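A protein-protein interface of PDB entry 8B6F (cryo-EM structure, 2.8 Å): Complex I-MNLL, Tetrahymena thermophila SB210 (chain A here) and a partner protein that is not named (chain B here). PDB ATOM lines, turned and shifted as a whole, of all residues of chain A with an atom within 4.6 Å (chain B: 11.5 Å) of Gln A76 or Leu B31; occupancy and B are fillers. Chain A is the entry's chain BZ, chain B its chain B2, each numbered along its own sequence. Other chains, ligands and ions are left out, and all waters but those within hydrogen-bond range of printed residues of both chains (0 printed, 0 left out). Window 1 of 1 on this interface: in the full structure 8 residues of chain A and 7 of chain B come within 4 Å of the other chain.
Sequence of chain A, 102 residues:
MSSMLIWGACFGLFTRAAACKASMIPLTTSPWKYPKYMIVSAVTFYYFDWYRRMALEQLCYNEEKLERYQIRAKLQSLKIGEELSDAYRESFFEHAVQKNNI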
ATOM      1  N   ARG A  72       9.348 -21.119  -0.142  1.00  0.00           N
ATOM      2  CA  ARG A  72       8.596 -21.339   1.088  1.00  0.00           C
ATOM      3  C   ARG A  72       7.099 -21.192   0.864  1.00  0.00           C
ATOM      4  O   ARG A  72       6.307 -21.881   1.514  1.00  0.00           O
ATOM      5  CB  ARG A  72       9.073 -20.375   2.171  1.00  0.00           C
ATOM      6  CG  ARG A  72      10.541 -20.535   2.511  1.00  0.00           C
ATOM      7  CD  ARG A  72      10.975 -19.567   3.592  1.00  0.00           C
ATOM      8  NE  ARG A  72      12.389 -19.721   3.910  1.00  0.00           N
ATOM      9  CZ  ARG A  72      13.037 -19.004   4.817  1.00  0.00           C
ATOM     10  NH1 ARG A  72      12.428 -18.066   5.522  1.00  0.00           N
ATOM     11  NH2 ARG A  72      14.329 -19.236   5.025  1.00  0.00           N
ATOM     12  N   ALA A  73       6.691 -20.303  -0.041  1.00  0.00           N
ATOM     13  CA  ALA A  73       5.276 -20.192  -0.372  1.00  0.00           C
ATOM     14  C   ALA A  73       4.764 -21.472  -1.022  1.00  0.00           C
ATOM     15  O   ALA A  73       3.638 -21.905  -0.757  1.00  0.00           O
ATOM     16  CB  ALA A  73       5.045 -18.995  -1.292  1.00  0.00           C
ATOM     17  N   LYS A  74       5.580 -22.087  -1.881  1.00  0.00           N
ATOM     18  CA  LYS A  74       5.176 -23.333  -2.523  1.00  0.00           C
ATOM     19  C   LYS A  74       4.957 -24.437  -1.498  1.00  0.00           C
ATOM     20  O   LYS A  74       3.976 -25.184  -1.581  1.00  0.00           O
ATOM     21  CB  LYS A  74       6.235 -23.752  -3.543  1.00  0.00           C
ATOM     22  CG  LYS A  74       5.913 -25.021  -4.318  1.00  0.00           C
ATOM     23  CD  LYS A  74       4.729 -24.823  -5.246  1.00  0.00           C
ATOM     24  CE  LYS A  74       4.510 -26.046  -6.122  1.00  0.00           C
ATOM     25  NZ  LYS A  74       3.412 -25.836  -7.104  1.00  0.00           N
ATOM     26  N   LEU A  75       5.861 -24.556  -0.525  1.00  0.00           N
ATOM     27  CA  LEU A  75       5.727 -25.603   0.483  1.00  0.00           C
ATOM     28  C   LEU A  75       4.482 -25.397   1.334  1.00  0.00           C
ATOM     29  O   LEU A  75       3.794 -26.362   1.683  1.00  0.00           O
ATOM     30  CB  LEU A  75       6.977 -25.648   1.361  1.00  0.00           C
ATOM     31  CG  LEU A  75       8.281 -26.039   0.662  1.00  0.00           C
ATOM     32  CD1 LEU A  75       9.446 -25.963   1.628  1.00  0.00           C
ATOM     33  CD2 LEU A  75       8.190 -27.430   0.062  1.00  0.00           C
ATOM     34  N   GLN A  76       4.180 -24.147   1.685  1.00  0.00           N
ATOM     35  CA  GLN A  76       2.988 -23.863   2.472  1.00  0.00           C
ATOM     36  C   GLN A  76       1.710 -23.977   1.652  1.00  0.00           C
ATOM     37  O   GLN A  76       0.635 -24.166   2.231  1.00  0.00           O
ATOM     38  CB  GLN A  76       3.088 -22.469   3.086  1.00  0.00           C
ATOM     39  CG  GLN A  76       4.255 -22.308   4.038  1.00  0.00           C
ATOM     40  CD  GLN A  76       4.347 -20.911   4.603  1.00  0.00           C
ATOM     41  OE1 GLN A  76       3.758 -20.610   5.639  1.00  0.00           O
ATOM     42  NE2 GLN A  76       5.089 -20.046   3.924  1.00  0.00           N
ATOM     43  N   SER A  77       1.800 -23.869   0.327  1.00  0.00           N
ATOM     44  CA  SER A  77       0.634 -24.031  -0.532  1.00  0.00           C
ATOM     45  C   SER A  77       0.271 -25.490  -0.769  1.00  0.00           C
ATOM     46  O   SER A  77      -0.793 -25.760  -1.335  1.00  0.00           O
ATOM     47  CB  SER A  77       0.879 -23.350  -1.881  1.00  0.00           C
ATOM     48  OG  SER A  77       1.150 -21.970  -1.716  1.00  0.00           O
ATOM     49  N   LEU A  78       1.121 -26.426  -0.356  1.00  0.00           N
ATOM     50  CA  LEU A  78       0.841 -27.838  -0.568  1.00  0.00           C
ATOM     51  C   LEU A  78      -0.485 -28.223   0.070  1.00  0.00           C
ATOM     52  O   LEU A  78      -0.797 -27.816   1.193  1.00  0.00           O
ATOM     53  CB  LEU A  78       1.968 -28.692   0.014  1.00  0.00           C
ATOM     54  CG  LEU A  78       3.358 -28.467  -0.580  1.00  0.00           C
ATOM     55  CD1 LEU A  78       4.397 -29.258   0.194  1.00  0.00           C
ATOM     56  CD2 LEU A  78       3.386 -28.843  -2.048  1.00  0.00           C
ATOM     57  N   PHE A  92      10.301 -30.529   2.681  1.00  0.00           N
ATOM     58  CA  PHE A  92       9.612 -29.988   3.845  1.00  0.00           C
ATOM     59  C   PHE A  92      10.461 -30.122   5.101  1.00  0.00           C
ATOM     60  O   PHE A  92      10.545 -29.188   5.906  1.00  0.00           O
ATOM     61  CB  PHE A  92       8.265 -30.684   4.026  1.00  0.00           C
ATOM     62  CG  PHE A  92       7.481 -30.181   5.198  1.00  0.00           C
ATOM     63  CD1 PHE A  92       6.626 -29.102   5.064  1.00  0.00           C
ATOM     64  CD2 PHE A  92       7.595 -30.793   6.435  1.00  0.00           C
ATOM     65  CE1 PHE A  92       5.903 -28.636   6.144  1.00  0.00           C
ATOM     66  CE2 PHE A  92       6.875 -30.333   7.519  1.00  0.00           C
ATOM     67  CZ  PHE A  92       6.027 -29.253   7.373  1.00  0.00           C
ATOM     68  N   HIS A  95      13.246 -27.512   5.065  1.00  0.00           N
ATOM     69  CA  HIS A  95      12.817 -26.166   5.423  1.00  0.00           C
ATOM     70  C   HIS A  95      12.277 -26.069   6.842  1.00  0.00           C
ATOM     71  O   HIS A  95      12.165 -24.957   7.368  1.00  0.00           O
ATOM     72  CB  HIS A  95      11.755 -25.675   4.440  1.00  0.00           C
ATOM     73  CG  HIS A  95      12.323 -25.122   3.171  1.00  0.00           C
ATOM     74  ND1 HIS A  95      12.730 -25.924   2.126  1.00  0.00           N
ATOM     75  CD2 HIS A  95      12.564 -23.849   2.783  1.00  0.00           C
ATOM     76  CE1 HIS A  95      13.191 -25.167   1.147  1.00  0.00           C
ATOM     77  NE2 HIS A  95      13.103 -23.904   1.520  1.00  0.00           N
ATOM     78  N   MET B  22       0.905 -17.659  19.205  1.00  0.00           N
ATOM     79  CA  MET B  22       0.731 -17.810  17.764  1.00  0.00           C
ATOM     80  C   MET B  22       1.632 -16.852  16.999  1.00  0.00           C
ATOM     81  O   MET B  22       2.273 -17.239  16.015  1.00  0.00           O
ATOM     82  CB  MET B  22      -0.732 -17.571  17.396  1.00  0.00           C
ATOM     83  CG  MET B  22      -1.035 -17.696  15.913  1.00  0.00           C
ATOM     84  SD  MET B  22      -2.742 -17.280  15.514  1.00  0.00           S
ATOM     85  CE  MET B  22      -2.790 -15.545  15.955  1.00  0.00           C
ATOM     86  N   LEU B  23       1.693 -15.593  17.434  1.00  0.00           N
ATOM     87  CA  LEU B  23       2.534 -14.619  16.748  1.00  0.00           C
ATOM     88  C   LEU B  23       4.007 -14.988  16.868  1.00  0.00           C
ATOM     89  O   LEU B  23       4.766 -14.859  15.901  1.00  0.00           O
ATOM     90  CB  LEU B  23       2.276 -13.222  17.307  1.00  0.00           C
ATOM     91  CG  LEU B  23       2.821 -12.055  16.482  1.00  0.00           C
ATOM     92  CD1 LEU B  23       2.200 -12.021  15.094  1.00  0.00           C
ATOM     93  CD2 LEU B  23       2.578 -10.744  17.200  1.00  0.00           C
ATOM     94  N   GLN B  24       4.431 -15.445  18.048  1.00  0.00           N
ATOM     95  CA  GLN B  24       5.818 -15.861  18.224  1.00  0.00           C
ATOM     96  C   GLN B  24       6.158 -17.015  17.290  1.00  0.00           C
ATOM     97  O   GLN B  24       7.210 -17.014  16.640  1.00  0.00           O
ATOM     98  CB  GLN B  24       6.054 -16.262  19.682  1.00  0.00           C
ATOM     99  CG  GLN B  24       7.516 -16.445  20.058  1.00  0.00           C
ATOM    100  CD  GLN B  24       8.222 -15.133  20.322  1.00  0.00           C
ATOM    101  OE1 GLN B  24       7.629 -14.060  20.210  1.00  0.00           O
ATOM    102  NE2 GLN B  24       9.500 -15.210  20.679  1.00  0.00           N
ATOM    103  N   CYS B  25       5.278 -18.015  17.213  1.00  0.00           N
ATOM    104  CA  CYS B  25       5.524 -19.147  16.326  1.00  0.00           C
ATOM    105  C   CYS B  25       5.566 -18.711  14.868  1.00  0.00           C
ATOM    106  O   CYS B  25       6.434 -19.151  14.105  1.00  0.00           O
ATOM    107  CB  CYS B  25       4.450 -20.217  16.523  1.00  0.00           C
ATOM    108  SG  CYS B  25       4.676 -21.668  15.465  1.00  0.00           S
ATOM    109  N   ALA B  26       4.638 -17.844  14.461  1.00  0.00           N
ATOM    110  CA  ALA B  26       4.612 -17.395  13.073  1.00  0.00           C
ATOM    111  C   ALA B  26       5.896 -16.667  12.706  1.00  0.00           C
ATOM    112  O   ALA B  26       6.445 -16.869  11.617  1.00  0.00           O
ATOM    113  CB  ALA B  26       3.400 -16.494  12.837  1.00  0.00           C
ATOM    114  N   LYS B  27       6.389 -15.809  13.598  1.00  0.00           N
ATOM    115  CA  LYS B  27       7.641 -15.110  13.331  1.00  0.00           C
ATOM    116  C   LYS B  27       8.814 -16.080  13.254  1.00  0.00           C
ATOM    117  O   LYS B  27       9.674 -15.955  12.375  1.00  0.00           O
ATOM    118  CB  LYS B  27       7.890 -14.063  14.414  1.00  0.00           C
ATOM    119  CG  LYS B  27       6.955 -12.872  14.376  1.00  0.00           C
ATOM    120  CD  LYS B  27       7.297 -11.899  15.491  1.00  0.00           C
ATOM    121  CE  LYS B  27       6.438 -10.655  15.426  1.00  0.00           C
ATOM    122  NZ  LYS B  27       6.804  -9.680  16.490  1.00  0.00           N
ATOM    123  N   SER B  28       8.869 -17.052  14.168  1.00  0.00           N
ATOM    124  CA  SER B  28      10.046 -17.912  14.258  1.00  0.00           C
ATOM    125  C   SER B  28      10.095 -18.922  13.117  1.00  0.00           C
ATOM    126  O   SER B  28      11.167 -19.180  12.558  1.00  0.00           O
ATOM    127  CB  SER B  28      10.066 -18.629  15.608  1.00  0.00           C
ATOM    128  OG  SER B  28       8.917 -19.442  15.773  1.00  0.00           O
ATOM    129  N   GLU B  29       8.956 -19.509  12.761  1.00  0.00           N
ATOM    130  CA  GLU B  29       8.950 -20.617  11.815  1.00  0.00           C
ATOM    131  C   GLU B  29       9.185 -20.129  10.391  1.00  0.00           C
ATOM    132  O   GLU B  29       8.714 -19.060   9.995  1.00  0.00           O
ATOM    133  CB  GLU B  29       7.620 -21.366  11.883  1.00  0.00           C
ATOM    134  CG  GLU B  29       7.338 -22.022  13.221  1.00  0.00           C
ATOM    135  CD  GLU B  29       8.303 -23.142  13.533  1.00  0.00           C
ATOM    136  OE1 GLU B  29       9.068 -23.537  12.629  1.00  0.00           O
ATOM    137  OE2 GLU B  29       8.299 -23.630  14.682  1.00  0.00           O
ATOM    138  N   ALA B  30       9.921 -20.931   9.616  1.00  0.00           N
ATOM    139  CA  ALA B  30      10.083 -20.675   8.191  1.00  0.00           C
ATOM    140  C   ALA B  30       8.856 -21.077   7.385  1.00  0.00           C
ATOM    141  O   ALA B  30       8.682 -20.592   6.263  1.00  0.00           O
ATOM    142  CB  ALA B  30      11.306 -21.419   7.657  1.00  0.00           C
ATOM    143  N   LEU B  31       8.012 -21.949   7.931  1.00  0.00           N
ATOM    144  CA  LEU B  31       6.756 -22.361   7.305  1.00  0.00           C
ATOM    145  C   LEU B  31       5.643 -22.154   8.321  1.00  0.00           C
ATOM    146  O   LEU B  31       5.058 -23.115   8.833  1.00  0.00           O
ATOM    147  CB  LEU B  31       6.816 -23.817   6.844  1.00  0.00           C
ATOM    148  CG  LEU B  31       7.925 -24.180   5.856  1.00  0.00           C
ATOM    149  CD1 LEU B  31       7.915 -25.672   5.584  1.00  0.00           C
ATOM    150  CD2 LEU B  31       7.778 -23.403   4.562  1.00  0.00           C
ATOM    151  N   PRO B  32       5.324 -20.899   8.638  1.00  0.00           N
ATOM    152  CA  PRO B  32       4.391 -20.642   9.744  1.00  0.00           C
ATOM    153  C   PRO B  32       3.023 -21.269   9.554  1.00  0.00           C
ATOM    154  O   PRO B  32       2.411 -21.700  10.537  1.00  0.00           O
ATOM    155  CB  PRO B  32       4.313 -19.108   9.780  1.00  0.00           C
ATOM    156  CG  PRO B  32       4.705 -18.670   8.416  1.00  0.00           C
ATOM    157  CD  PRO B  32       5.726 -19.659   7.950  1.00  0.00           C
ATOM    158  N   ILE B  33       2.522 -21.338   8.321  1.00  0.00           N
ATOM    159  CA  ILE B  33       1.171 -21.847   8.100  1.00  0.00           C
ATOM    160  C   ILE B  33       1.068 -23.301   8.533  1.00  0.00           C
ATOM    161  O   ILE B  33       0.086 -23.706   9.168  1.00  0.00           O
ATOM    162  CB  ILE B  33       0.764 -21.664   6.625  1.00  0.00           C
ATOM    163  CG1 ILE B  33       0.684 -20.177   6.269  1.00  0.00           C
ATOM    164  CG2 ILE B  33      -0.570 -22.352   6.338  1.00  0.00           C
ATOM    165  CD1 ILE B  33      -0.259 -19.372   7.136  1.00  0.00           C
ATOM    166  N   LYS B  34       2.069 -24.110   8.198  1.00  0.00           N
ATOM    167  CA  LYS B  34       2.026 -25.531   8.508  1.00  0.00           C
ATOM    168  C   LYS B  34       2.650 -25.866   9.854  1.00  0.00           C
ATOM    169  O   LYS B  34       2.274 -26.874  10.464  1.00  0.00           O
ATOM    170  CB  LYS B  34       2.727 -26.332   7.408  1.00  0.00           C
ATOM    171  CG  LYS B  34       2.010 -26.278   6.071  1.00  0.00           C
ATOM    172  CD  LYS B  34       2.508 -27.364   5.136  1.00  0.00           C
ATOM    173  CE  LYS B  34       1.755 -27.352   3.816  1.00  0.00           C
ATOM    174  NZ  LYS B  34       0.294 -27.571   3.990  1.00  0.00           N
ATOM    175  N   MET B  35       3.585 -25.052  10.336  1.00  0.00           N
ATOM    176  CA  MET B  35       4.317 -25.358  11.556  1.00  0.00           C
ATOM    177  C   MET B  35       3.779 -24.643  12.788  1.00  0.00           C
ATOM    178  O   MET B  35       4.345 -24.810  13.873  1.00  0.00           O
ATOM    179  CB  MET B  35       5.798 -25.016  11.383  1.00  0.00           C
ATOM    180  CG  MET B  35       6.516 -25.863  10.351  1.00  0.00           C
ATOM    181  SD  MET B  35       6.239 -27.628  10.589  1.00  0.00           S
ATOM    182  CE  MET B  35       6.526 -27.788  12.351  1.00  0.00           C
ATOM    183  N   CYS B  36       2.713 -23.859  12.658  1.00  0.00           N
ATOM    184  CA  CYS B  36       2.085 -23.205  13.799  1.00  0.00           C
ATOM    185  C   CYS B  36       0.623 -23.615  13.932  1.00  0.00           C
ATOM    186  O   CYS B  36      -0.198 -22.862  14.456  1.00  0.00           O
ATOM    187  CB  CYS B  36       2.212 -21.687  13.695  1.00  0.00           C
ATOM    188  SG  CYS B  36       3.923 -21.122  13.655  1.00  0.00           S
ATOM    189  N   THR B  37       0.289 -24.813  13.451  1.00  0.00           N
ATOM    190  CA  THR B  37      -1.094 -25.270  13.501  1.00  0.00           C
ATOM    191  C   THR B  37      -1.591 -25.369  14.937  1.00  0.00           C
ATOM    192  O   THR B  37      -2.723 -24.972  15.238  1.00  0.00           O
ATOM    193  CB  THR B  37      -1.221 -26.621  12.796  1.00  0.00           C
ATOM    194  OG1 THR B  37      -0.300 -27.554  13.374  1.00  0.00           O
ATOM    195  CG2 THR B  37      -0.925 -26.478  11.314  1.00  0.00           C
ATOM    196  N   ALA B  38      -0.764 -25.899  15.840  1.00  0.00           N
ATOM    197  CA  ALA B  38      -1.197 -26.075  17.222  1.00  0.00           C
ATOM    198  C   ALA B  38      -1.520 -24.738  17.875  1.00  0.00           C
ATOM    199  O   ALA B  38      -2.599 -24.559  18.451  1.00  0.00           O
ATOM    200  CB  ALA B  38      -0.120 -26.813  18.017  1.00  0.00           C
ATOM    201  N   GLN B  39      -0.594 -23.779  17.793  1.00  0.00           N
ATOM    202  CA  GLN B  39      -0.829 -22.480  18.415  1.00  0.00           C
ATOM    203  C   GLN B  39      -2.013 -21.766  17.780  1.00  0.00           C
ATOM    204  O   GLN B  39      -2.843 -21.179  18.483  1.00  0.00           O
ATOM    205  CB  GLN B  39       0.426 -21.613  18.321  1.00  0.00           C
ATOM    206  CG  GLN B  39       1.559 -22.054  19.233  1.00  0.00           C
ATOM    207  CD  GLN B  39       2.327 -23.240  18.700  1.00  0.00           C
ATOM    208  OE1 GLN B  39       2.269 -23.553  17.513  1.00  0.00           O
ATOM    209  NE2 GLN B  39       3.053 -23.913  19.583  1.00  0.00           N
ATOM    210  N   THR B  40      -2.107 -21.801  16.452  1.00  0.00           N
ATOM    211  CA  THR B  40      -3.202 -21.117  15.774  1.00  0.00           C
ATOM    212  C   THR B  40      -4.545 -21.735  16.131  1.00  0.00           C
ATOM    213  O   THR B  40      -5.535 -21.020  16.323  1.00  0.00           O
ATOM    214  CB  THR B  40      -2.996 -21.126  14.265  1.00  0.00           C
ATOM    215  OG1 THR B  40      -1.676 -20.666  13.951  1.00  0.00           O
ATOM    216  CG2 THR B  40      -3.998 -20.189  13.632  1.00  0.00           C
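Gln A76 touches just these residues of chain B: Leu B31, Pro B32, Ile B33 and Lys B34.
Of the printed residues of chain A, Leu B31 touches Arg A72 (3.7 Å), Leu A75 (3.99 Å), Gln A76 (3.6 Å) and Phe A92 (3.6 Å).
Ala A73 touches none of the printed residues of chain B.
No residue of chain B comes within 4 Å of Ser A77.
Leu A78 touches just one residue of chain B: Lys B34.
Phe A92 touches just these residues of chain B: Leu B31, Lys B34 and Met B35.
Printed residues of chain B within 4 Å of His A95: Ala B30 (3.7 Å).
Of the printed residues of chain A, Lys B34 touches Leu A75 (3.1 Å), Gln A76 (3.7 Å), Leu A78 (3.0 Å) and Phe A92 (3.8 Å).
Of the printed residues of chain B, Leu A75 touches Leu B31 (3.99 Å) and Lys B34 (3.1 Å).
Of the printed residues of chain A, Pro B32 touches Gln A76.
Glu B29 touches none of the printed residues of chain A.
The nearest printed residue of chain A that does not touch Leu B31 is His A95 (4.01 Å).
The nearest printed residue of chain B that does not touch Leu A75 is Ala B30 (7.1 Å).
Of the 19 printed residues of chain B, 6 touch a printed residue of chain A.
Hydrophobic or aromatic side chains of chain B that line the printed part of chain A: Ala B30, Leu B31, Pro B32, Ile B33 and Met B35.
Printed residues of chain A that touch a printed residue of chain B: Arg A72, Leu A75, Gln A76, Leu A78, Phe A92 and His A95.
Hydrophobic or aromatic side chains of chain A within 4 Å of the printed part of chain B: Leu A75 and Phe A92.
Among the printed residues, no Asp or Glu carboxylate lies within 4 Å of a Lys or Arg side-chain nitrogen of the other chain.
The side-chain amide oxygen (OE1) of Gln A76 lies close to the backbone nitrogen (N) of Pro B32 (3.4 Å).
NZ of Lys B34 is in hydrogen-bond range of O of Leu A78, at 3.0 Å.
The backbone NH (N) of Ile B33 lies within hydrogen-bond range of the side-chain amide oxygen (OE1) of Gln A76 (3.0 Å).
The backbone carbonyl oxygen of Arg A72 is in hydrogen-bond range of the side-chain amide nitrogen of Gln A76 (3.3 Å).
SG of Cys B25 is disulfide-bonded to SG of Cys B36.
Among the printed residues, pairs that only touch across the chains: Arg A72 with Ala B30, Arg A72 with Leu B31, Leu A75 with Leu B31, Leu A75 with Lys B34, Gln A76 with Leu B31, Gln A76 with Lys B34, Phe A92 with Leu B31, Phe A92 with Lys B34, Phe A92 with Met B35 and His A95 with Ala B30.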
